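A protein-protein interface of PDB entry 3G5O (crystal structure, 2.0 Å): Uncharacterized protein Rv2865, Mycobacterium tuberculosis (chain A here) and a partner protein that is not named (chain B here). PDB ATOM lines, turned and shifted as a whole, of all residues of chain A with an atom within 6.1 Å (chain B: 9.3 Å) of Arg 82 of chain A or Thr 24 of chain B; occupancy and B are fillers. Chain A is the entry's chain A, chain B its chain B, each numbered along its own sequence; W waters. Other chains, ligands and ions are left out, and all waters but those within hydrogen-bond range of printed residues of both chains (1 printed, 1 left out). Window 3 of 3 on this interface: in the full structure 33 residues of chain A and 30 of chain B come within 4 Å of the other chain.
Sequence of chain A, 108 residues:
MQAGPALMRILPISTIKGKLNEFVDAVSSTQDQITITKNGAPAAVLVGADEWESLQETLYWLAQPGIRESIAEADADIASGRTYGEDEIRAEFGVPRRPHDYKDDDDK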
ATOM      1  N   GLU A  73     -22.971  -6.738  13.476  1.00  0.00           N
ATOM      2  CA  GLU A  73     -22.204  -7.971  13.681  1.00  0.00           C
ATOM      3  C   GLU A  73     -21.129  -8.161  12.597  1.00  0.00           C
ATOM      4  O   GLU A  73     -19.976  -8.508  12.878  1.00  0.00           O
ATOM      5  CB  GLU A  73     -23.132  -9.192  13.692  1.00  0.00           C
ATOM      6  CG  GLU A  73     -23.892  -9.421  14.996  1.00  0.00           C
ATOM      7  CD  GLU A  73     -24.745 -10.711  14.971  1.00  0.00           C
ATOM      8  OE1 GLU A  73     -24.186 -11.809  14.693  1.00  0.00           O
ATOM      9  OE2 GLU A  73     -25.976 -10.616  15.226  1.00  0.00           O
ATOM     10  N   ALA A  76     -18.385  -5.678  13.332  1.00  0.00           N
ATOM     11  CA  ALA A  76     -17.506  -6.207  14.383  1.00  0.00           C
ATOM     12  C   ALA A  76     -16.561  -7.301  13.877  1.00  0.00           C
ATOM     13  O   ALA A  76     -15.389  -7.334  14.287  1.00  0.00           O
ATOM     14  CB  ALA A  76     -18.281  -6.638  15.685  1.00  0.00           C
ATOM     15  N   ASP A  77     -17.033  -8.154  12.949  1.00  0.00           N
ATOM     16  CA  ASP A  77     -16.132  -9.122  12.283  1.00  0.00           C
ATOM     17  C   ASP A  77     -15.019  -8.394  11.551  1.00  0.00           C
ATOM     18  O   ASP A  77     -13.823  -8.766  11.673  1.00  0.00           O
ATOM     19  CB  ASP A  77     -16.845 -10.017  11.273  1.00  0.00           C
ATOM     20  CG  ASP A  77     -17.909 -10.911  11.903  1.00  0.00           C
ATOM     21  OD1 ASP A  77     -17.816 -11.300  13.126  1.00  0.00           O
ATOM     22  OD2 ASP A  77     -18.865 -11.240  11.144  1.00  0.00           O
ATOM     23  N   ILE A  78     -15.396  -7.360  10.788  1.00  0.00           N
ATOM     24  CA  ILE A  78     -14.399  -6.650  10.043  1.00  0.00           C
ATOM     25  C   ILE A  78     -13.328  -6.103  10.997  1.00  0.00           C
ATOM     26  O   ILE A  78     -12.141  -6.246  10.716  1.00  0.00           O
ATOM     27  CB  ILE A  78     -14.983  -5.519   9.199  1.00  0.00           C
ATOM     28  CG1 ILE A  78     -15.769  -6.099   8.010  1.00  0.00           C
ATOM     29  CG2 ILE A  78     -13.847  -4.585   8.712  1.00  0.00           C
ATOM     30  CD1 ILE A  78     -16.633  -5.080   7.319  1.00  0.00           C
ATOM     31  N   ALA A  79     -13.750  -5.513  12.108  1.00  0.00           N
ATOM     32  CA  ALA A  79     -12.813  -4.866  13.048  1.00  0.00           C
ATOM     33  C   ALA A  79     -11.911  -5.873  13.774  1.00  0.00           C
ATOM     34  O   ALA A  79     -10.834  -5.491  14.234  1.00  0.00           O
ATOM     35  CB  ALA A  79     -13.557  -3.954  14.081  1.00  0.00           C
ATOM     36  N   SER A  80     -12.345  -7.140  13.871  1.00  0.00           N
ATOM     37  CA  SER A  80     -11.558  -8.196  14.505  1.00  0.00           C
ATOM     38  C   SER A  80     -10.796  -9.078  13.501  1.00  0.00           C
ATOM     39  O   SER A  80     -10.153 -10.012  13.906  1.00  0.00           O
ATOM     40  CB  SER A  80     -12.472  -9.117  15.325  1.00  0.00           C
ATOM     41  OG  SER A  80     -12.813  -8.532  16.563  1.00  0.00           O
ATOM     42  N   GLY A  81     -10.916  -8.806  12.204  1.00  0.00           N
ATOM     43  CA  GLY A  81     -10.374  -9.708  11.176  1.00  0.00           C
ATOM     44  C   GLY A  81     -11.075 -11.076  11.090  1.00  0.00           C
ATOM     45  O   GLY A  81     -10.458 -12.038  10.641  1.00  0.00           O
ATOM     46  N   ARG A  82     -12.361 -11.163  11.467  1.00  0.00           N
ATOM     47  CA  ARG A  82     -13.104 -12.439  11.288  1.00  0.00           C
ATOM     48  C   ARG A  82     -13.712 -12.454   9.855  1.00  0.00           C
ATOM     49  O   ARG A  82     -14.911 -12.223   9.671  1.00  0.00           O
ATOM     50  CB  ARG A  82     -14.208 -12.618  12.339  1.00  0.00           C
ATOM     51  CG  ARG A  82     -13.697 -12.749  13.790  1.00  0.00           C
ATOM     52  CD  ARG A  82     -14.846 -13.157  14.745  1.00  0.00           C
ATOM     53  NE  ARG A  82     -15.792 -12.047  14.935  1.00  0.00           N
ATOM     54  CZ  ARG A  82     -15.739 -11.198  15.964  1.00  0.00           C
ATOM     55  NH1 ARG A  82     -14.776 -11.332  16.888  1.00  0.00           N
ATOM     56  NH2 ARG A  82     -16.632 -10.220  16.075  1.00  0.00           N
ATOM     57  N   THR A  83     -12.854 -12.664   8.871  1.00  0.00           N
ATOM     58  CA  THR A  83     -13.253 -12.743   7.468  1.00  0.00           C
ATOM     59  C   THR A  83     -12.482 -13.872   6.820  1.00  0.00           C
ATOM     60  O   THR A  83     -11.461 -14.341   7.372  1.00  0.00           O
ATOM     61  CB  THR A  83     -12.956 -11.447   6.692  1.00  0.00           C
ATOM     62  OG1 THR A  83     -11.536 -11.243   6.712  1.00  0.00           O
ATOM     63  CG2 THR A  83     -13.664 -10.222   7.318  1.00  0.00           C
ATOM     64  N   TYR A  84     -12.983 -14.310   5.663  1.00  0.00           N
ATOM     65  CA  TYR A  84     -12.485 -15.476   4.929  1.00  0.00           C
ATOM     66  C   TYR A  84     -12.322 -15.097   3.465  1.00  0.00           C
ATOM     67  O   TYR A  84     -13.180 -14.390   2.895  1.00  0.00           O
ATOM     68  CB  TYR A  84     -13.484 -16.661   5.049  1.00  0.00           C
ATOM     69  CG  TYR A  84     -13.625 -17.108   6.500  1.00  0.00           C
ATOM     70  CD1 TYR A  84     -12.828 -18.136   7.009  1.00  0.00           C
ATOM     71  CD2 TYR A  84     -14.491 -16.440   7.365  1.00  0.00           C
ATOM     72  CE1 TYR A  84     -12.922 -18.506   8.354  1.00  0.00           C
ATOM     73  CE2 TYR A  84     -14.630 -16.811   8.685  1.00  0.00           C
ATOM     74  CZ  TYR A  84     -13.835 -17.836   9.187  1.00  0.00           C
ATOM     75  OH  TYR A  84     -13.948 -18.163  10.524  1.00  0.00           O
ATOM     76  N   ARG B  21     -13.583 -10.767   0.477  1.00  0.00           N
ATOM     77  CA  ARG B  21     -13.612 -11.473   1.745  1.00  0.00           C
ATOM     78  C   ARG B  21     -15.072 -11.607   2.197  1.00  0.00           C
ATOM     79  O   ARG B  21     -15.900 -10.689   1.945  1.00  0.00           O
ATOM     80  CB  ARG B  21     -12.884 -10.654   2.821  1.00  0.00           C
ATOM     81  CG  ARG B  21     -11.435 -10.240   2.440  1.00  0.00           C
ATOM     82  CD  ARG B  21     -10.490 -11.401   2.530  1.00  0.00           C
ATOM     83  NE  ARG B  21     -10.294 -11.882   3.915  1.00  0.00           N
ATOM     84  CZ  ARG B  21      -9.417 -12.838   4.237  1.00  0.00           C
ATOM     85  NH1 ARG B  21      -8.688 -13.426   3.290  1.00  0.00           N
ATOM     86  NH2 ARG B  21      -9.289 -13.210   5.495  1.00  0.00           N
ATOM     87  N   PHE B  22     -15.378 -12.721   2.864  1.00  0.00           N
ATOM     88  CA  PHE B  22     -16.648 -12.881   3.540  1.00  0.00           C
ATOM     89  C   PHE B  22     -16.450 -12.755   5.033  1.00  0.00           C
ATOM     90  O   PHE B  22     -15.566 -13.429   5.570  1.00  0.00           O
ATOM     91  CB  PHE B  22     -17.227 -14.305   3.258  1.00  0.00           C
ATOM     92  CG  PHE B  22     -17.899 -14.435   1.911  1.00  0.00           C
ATOM     93  CD1 PHE B  22     -19.279 -14.351   1.812  1.00  0.00           C
ATOM     94  CD2 PHE B  22     -17.134 -14.562   0.736  1.00  0.00           C
ATOM     95  CE1 PHE B  22     -19.916 -14.491   0.570  1.00  0.00           C
ATOM     96  CE2 PHE B  22     -17.748 -14.682  -0.546  1.00  0.00           C
ATOM     97  CZ  PHE B  22     -19.166 -14.670  -0.616  1.00  0.00           C
ATOM     98  N   THR B  23     -17.271 -11.925   5.706  1.00  0.00           N
ATOM     99  CA  THR B  23     -17.366 -11.926   7.170  1.00  0.00           C
ATOM    100  C   THR B  23     -17.927 -13.231   7.685  1.00  0.00           C
ATOM    101  O   THR B  23     -18.655 -13.937   6.968  1.00  0.00           O
ATOM    102  CB  THR B  23     -18.262 -10.791   7.731  1.00  0.00           C
ATOM    103  OG1 THR B  23     -19.585 -10.943   7.180  1.00  0.00           O
ATOM    104  CG2 THR B  23     -17.680  -9.400   7.377  1.00  0.00           C
ATOM    105  N   THR B  24     -17.598 -13.556   8.939  1.00  0.00           N
ATOM    106  CA  THR B  24     -18.189 -14.704   9.615  1.00  0.00           C
ATOM    107  C   THR B  24     -19.717 -14.649   9.512  1.00  0.00           C
ATOM    108  O   THR B  24     -20.358 -15.650   9.243  1.00  0.00           O
ATOM    109  CB  THR B  24     -17.736 -14.764  11.076  1.00  0.00           C
ATOM    110  OG1 THR B  24     -16.307 -14.789  11.085  1.00  0.00           O
ATOM    111  CG2 THR B  24     -18.243 -16.038  11.760  1.00  0.00           C
ATOM    112  N   THR B  25     -20.271 -13.456   9.689  1.00  0.00           N
ATOM    113  CA  THR B  25     -21.697 -13.225   9.601  1.00  0.00           C
ATOM    114  C   THR B  25     -22.239 -13.657   8.221  1.00  0.00           C
ATOM    115  O   THR B  25     -23.193 -14.413   8.142  1.00  0.00           O
ATOM    116  CB  THR B  25     -22.003 -11.739   9.940  1.00  0.00           C
ATOM    117  OG1 THR B  25     -21.548 -11.501  11.274  1.00  0.00           O
ATOM    118  CG2 THR B  25     -23.522 -11.428   9.868  1.00  0.00           C
ATOM    119  N   ALA B  26     -21.579 -13.224   7.146  1.00  0.00           N
ATOM    120  CA  ALA B  26     -22.011 -13.565   5.781  1.00  0.00           C
ATOM    121  C   ALA B  26     -21.800 -15.051   5.462  1.00  0.00           C
ATOM    122  O   ALA B  26     -22.601 -15.658   4.734  1.00  0.00           O
ATOM    123  CB  ALA B  26     -21.296 -12.663   4.743  1.00  0.00           C
ATOM    124  N   ARG B  27     -20.739 -15.640   6.026  1.00  0.00           N
ATOM    125  CA  ARG B  27     -20.501 -17.073   5.907  1.00  0.00           C
ATOM    126  C   ARG B  27     -21.666 -17.914   6.474  1.00  0.00           C
ATOM    127  O   ARG B  27     -22.051 -18.897   5.864  1.00  0.00           O
ATOM    128  CB  ARG B  27     -19.151 -17.470   6.521  1.00  0.00           C
ATOM    129  CG  ARG B  27     -18.762 -18.928   6.184  1.00  0.00           C
ATOM    130  CD  ARG B  27     -17.421 -19.334   6.769  1.00  0.00           C
ATOM    131  NE  ARG B  27     -17.458 -19.368   8.218  1.00  0.00           N
ATOM    132  CZ  ARG B  27     -16.626 -20.072   8.986  1.00  0.00           C
ATOM    133  NH1 ARG B  27     -15.682 -20.838   8.454  1.00  0.00           N
ATOM    134  NH2 ARG B  27     -16.737 -19.990  10.307  1.00  0.00           N
ATOM    135  N   ARG B  28     -22.208 -17.519   7.634  1.00  0.00           N
ATOM    136  CA  ARG B  28     -23.421 -18.119   8.190  1.00  0.00           C
ATOM    137  C   ARG B  28     -24.570 -18.083   7.178  1.00  0.00           C
ATOM    138  O   ARG B  28     -25.342 -19.041   7.073  1.00  0.00           O
ATOM    139  CB  ARG B  28     -23.896 -17.400   9.479  1.00  0.00           C
ATOM    140  CG  ARG B  28     -23.125 -17.707  10.772  1.00  0.00           C
ATOM    141  CD  ARG B  28     -23.899 -17.223  12.063  1.00  0.00           C
ATOM    142  NE  ARG B  28     -23.798 -15.768  12.281  1.00  0.00           N
ATOM    143  CZ  ARG B  28     -22.686 -15.129  12.682  1.00  0.00           C
ATOM    144  NH1 ARG B  28     -21.558 -15.794  12.907  1.00  0.00           N
ATOM    145  NH2 ARG B  28     -22.692 -13.806  12.839  1.00  0.00           N
ATOM    146  N   ASP B  29     -24.698 -16.965   6.469  1.00  0.00           N
ATOM    147  CA  ASP B  29     -25.717 -16.843   5.394  1.00  0.00           C
ATOM    148  C   ASP B  29     -25.489 -17.844   4.280  1.00  0.00           C
ATOM    149  O   ASP B  29     -26.442 -18.415   3.743  1.00  0.00           O
ATOM    150  CB  ASP B  29     -25.698 -15.438   4.778  1.00  0.00           C
ATOM    151  CG  ASP B  29     -26.221 -14.386   5.727  1.00  0.00           C
ATOM    152  OD1 ASP B  29     -26.866 -14.758   6.720  1.00  0.00           O
ATOM    153  OD2 ASP B  29     -25.972 -13.186   5.497  1.00  0.00           O
ATOM    154  N   LEU B  30     -24.228 -18.038   3.915  1.00  0.00           N
ATOM    155  CA  LEU B  30     -23.875 -19.012   2.861  1.00  0.00           C
ATOM    156  C   LEU B  30     -24.327 -20.423   3.172  1.00  0.00           C
ATOM    157  O   LEU B  30     -24.789 -21.131   2.277  1.00  0.00           O
ATOM    158  CB  LEU B  30     -22.373 -19.015   2.585  1.00  0.00           C
ATOM    159  CG  LEU B  30     -21.799 -17.839   1.788  1.00  0.00           C
ATOM    160  CD1 LEU B  30     -20.268 -18.103   1.689  1.00  0.00           C
ATOM    161  CD2 LEU B  30     -22.368 -17.706   0.402  1.00  0.00           C
ATOM    162  N   HIS B  31     -24.238 -20.805   4.454  1.00  0.00           N
ATOM    163  CA  HIS B  31     -24.635 -22.131   4.908  1.00  0.00           C
ATOM    164  C   HIS B  31     -26.107 -22.407   4.762  1.00  0.00           C
ATOM    165  O   HIS B  31     -26.504 -23.570   4.797  1.00  0.00           O
ATOM    166  CB  HIS B  31     -24.209 -22.389   6.367  1.00  0.00           C
ATOM    167  CG  HIS B  31     -22.809 -22.905   6.500  1.00  0.00           C
ATOM    168  ND1 HIS B  31     -22.445 -24.182   6.116  1.00  0.00           N
ATOM    169  CD2 HIS B  31     -21.679 -22.312   6.956  1.00  0.00           C
ATOM    170  CE1 HIS B  31     -21.147 -24.350   6.329  1.00  0.00           C
ATOM    171  NE2 HIS B  31     -20.661 -23.230   6.847  1.00  0.00           N
ATOM    172  N   VAL B  89     -15.720  -6.449   1.185  1.00  0.00           N
ATOM    173  CA  VAL B  89     -16.082  -7.332   2.288  1.00  0.00           C
ATOM    174  C   VAL B  89     -17.588  -7.549   2.291  1.00  0.00           C
ATOM    175  O   VAL B  89     -18.341  -6.580   2.317  1.00  0.00           O
ATOM    176  CB  VAL B  89     -15.623  -6.766   3.680  1.00  0.00           C
ATOM    177  CG1 VAL B  89     -15.960  -7.754   4.772  1.00  0.00           C
ATOM    178  CG2 VAL B  89     -14.135  -6.510   3.703  1.00  0.00           C
ATOM    179  N   ILE B  90     -18.016  -8.819   2.268  1.00  0.00           N
ATOM    180  CA  ILE B  90     -19.439  -9.178   2.186  1.00  0.00           C
ATOM    181  C   ILE B  90     -19.992  -9.207   3.602  1.00  0.00           C
ATOM    182  O   ILE B  90     -19.432  -9.865   4.470  1.00  0.00           O
ATOM    183  CB  ILE B  90     -19.662 -10.576   1.507  1.00  0.00           C
ATOM    184  CG1 ILE B  90     -18.900 -10.674   0.188  1.00  0.00           C
ATOM    185  CG2 ILE B  90     -21.162 -10.853   1.264  1.00  0.00           C
ATOM    186  CD1 ILE B  90     -19.165  -9.533  -0.728  1.00  0.00           C
ATOM    187  N   LEU B  91     -21.072  -8.480   3.825  1.00  0.00           N
ATOM    188  CA  LEU B  91     -21.744  -8.417   5.106  1.00  0.00           C
ATOM    189  C   LEU B  91     -22.914  -9.401   5.233  1.00  0.00           C
ATOM    190  O   LEU B  91     -23.132  -9.984   6.298  1.00  0.00           O
ATOM    191  CB  LEU B  91     -22.253  -6.991   5.311  1.00  0.00           C
ATOM    192  CG  LEU B  91     -21.298  -5.793   5.130  1.00  0.00           C
ATOM    193  CD1 LEU B  91     -22.038  -4.520   5.562  1.00  0.00           C
ATOM    194  CD2 LEU B  91     -19.926  -5.915   5.896  1.00  0.00           C
ATOM    195  N   ARG B  92     -23.660  -9.590   4.147  1.00  0.00           N
ATOM    196  CA  ARG B  92     -24.879 -10.394   4.188  1.00  0.00           C
ATOM    197  C   ARG B  92     -25.175 -10.939   2.804  1.00  0.00           C
ATOM    198  O   ARG B  92     -24.847 -10.293   1.796  1.00  0.00           O
ATOM    199  CB  ARG B  92     -26.064  -9.559   4.712  1.00  0.00           C
ATOM    200  CG  ARG B  92     -27.394 -10.377   4.924  1.00  0.00           C
ATOM    201  CD  ARG B  92     -28.295  -9.751   6.050  1.00  0.00           C
ATOM    202  NE  ARG B  92     -29.695 -10.186   5.924  1.00  0.00           N
ATOM    203  CZ  ARG B  92     -30.658 -10.003   6.843  1.00  0.00           C
ATOM    204  NH1 ARG B  92     -30.397  -9.396   8.003  1.00  0.00           N
ATOM    205  NH2 ARG B  92     -31.889 -10.451   6.612  1.00  0.00           N
ATOM    206  N   VAL B  93     -25.692 -12.162   2.757  1.00  0.00           N
ATOM    207  CA  VAL B  93     -26.185 -12.745   1.515  1.00  0.00           C
ATOM    208  C   VAL B  93     -27.654 -13.117   1.734  1.00  0.00           C
ATOM    209  O   VAL B  93     -27.993 -13.855   2.668  1.00  0.00           O
ATOM    210  CB  VAL B  93     -25.392 -13.975   1.124  1.00  0.00           C
ATOM    211  CG1 VAL B  93     -25.869 -14.565  -0.259  1.00  0.00           C
ATOM    212  CG2 VAL B  93     -23.852 -13.669   1.148  1.00  0.00           C
HETATM  213  O   HOH W   1     -14.880 -16.372  12.593  1.00  0.00           O
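Of chain B, only Thr 23 and Thr 24 come within 4 Å of Arg 82 of chain A.
Thr 24 of chain B touches just these residues of chain A: Asp 77 (3.4 Å), Arg 82 (3.1 Å) and Tyr 84 (3.6 Å).
Printed residues of chain B within 4 Å of Asp 77 of chain A: Thr 23, Thr 24 and Thr 25.
No residue of chain B comes within 4 Å of Ser 80 of chain A.
Of chain B, only Arg 21 and Phe 22 come within 4 Å of Thr 83 of chain A.
Printed residues of chain A within 4 Å of Thr 23 of chain B: Asp 77 (3.5 Å), Ile 78 (3.9 Å) and Arg 82 (3.5 Å).
Of the printed residues of chain A, Thr 25 of chain B touches Glu 73 (3.6 Å) and Asp 77 (2.7 Å).
Of the printed residues of chain A, Arg 27 of chain B touches Tyr 84.
Of the printed residues of chain B, Tyr 84 of chain A touches Arg 21 (3.2 Å), Phe 22 (2.7 Å), Thr 24 (3.6 Å) and Arg 27 (3.3 Å).
Asp 29 of chain B touches none of the printed residues of chain A.
The nearest residue of chain B that does not touch Arg 82 of chain A is Phe 22 of chain B (4.3 Å).
Hydrophobic or aromatic side chains of chain B that line the printed part of chain A: Val 89 and Leu 91.
Hydrophobic or aromatic side chains of chain A within 4 Å of the printed part of chain B: Ile 78 and Tyr 84.
Water W1 bridges the side-chain hydroxyl (OG1) of Thr 24 of chain B (2.6 Å) and the side-chain hydroxyl (OH) of Tyr 84 of chain A (2.9 Å).
OD2 of Asp 77 of chain A sits at hydrogen-bond distance from OG1 of Thr 25 of chain B (2.7 Å).
The backbone carbonyl oxygen (O) of Phe 22 of chain B lies within hydrogen-bond range of the backbone NH (N) of Tyr 84 of chain A, at 2.7 Å.
N of Thr 24 of chain B sits at hydrogen-bond distance from O of Arg 82 of chain A (3.1 Å).
The backbone carbonyl oxygen (O) of Thr 83 of chain A lies within hydrogen-bond range of the guanidinium group (NH2) of Arg 21 of chain B (3.1 Å).
The guanidinium group (NH2) of Arg 27 of chain B is in hydrogen-bond range of the side-chain hydroxyl (OH) of Tyr 84 of chain A (3.3 Å).
The backbone NH (N) of Thr 24 of chain B sits at hydrogen-bond distance from the side-chain carboxylate (OD2) of Asp 77 of chain A.
OE1 of Glu 73 of chain A lies within salt-bridge range of NH2 of Arg 28 of chain B (3.1 Å).
Among the printed residues, pairs that only touch across the chains: Thr 83 of chain A with Phe 22 of chain B, Tyr 84 of chain A with Arg 21 of chain B, Asp 77 of chain A with Thr 23 of chain B, Arg 82 of chain A with Thr 23 of chain B, Tyr 84 of chain A with Thr 24 of chain B, Glu 73 of chain A with Thr 25 of chain B, Ile 78 of chain A with Val 89 of chain B, Ile 78 of chain A with Leu 91 of chain B and Ile 78 of chain A with Thr 23 of chain B.
The side-chain hydroxyl of Thr 25 of chain B lies within hydrogen-bond range of the guanidinium group of Arg 28 of chain B (3.0 Å).
OG of Ser 80 of chain A sits at hydrogen-bond distance from NH1 of Arg 82 of chain A, 3.4 Å away.
The backbone carbonyl oxygen (O) of Arg 21 of chain B is in hydrogen-bond range of the backbone NH (N) of Ile 90 of chain B, at 2.8 Å.
OD1 of Asp 77 of chain A lies within salt-bridge range of NE of Arg 82 of chain A (2.8 Å).
OG1 of Thr 23 of chain B is in hydrogen-bond range of N of Ala 26 of chain B, at 3.0 Å.
The side-chain hydroxyl of Thr 23 of chain B lies within hydrogen-bond range of the backbone carbonyl oxygen of Ile 90 of chain B, 2.9 Å away.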
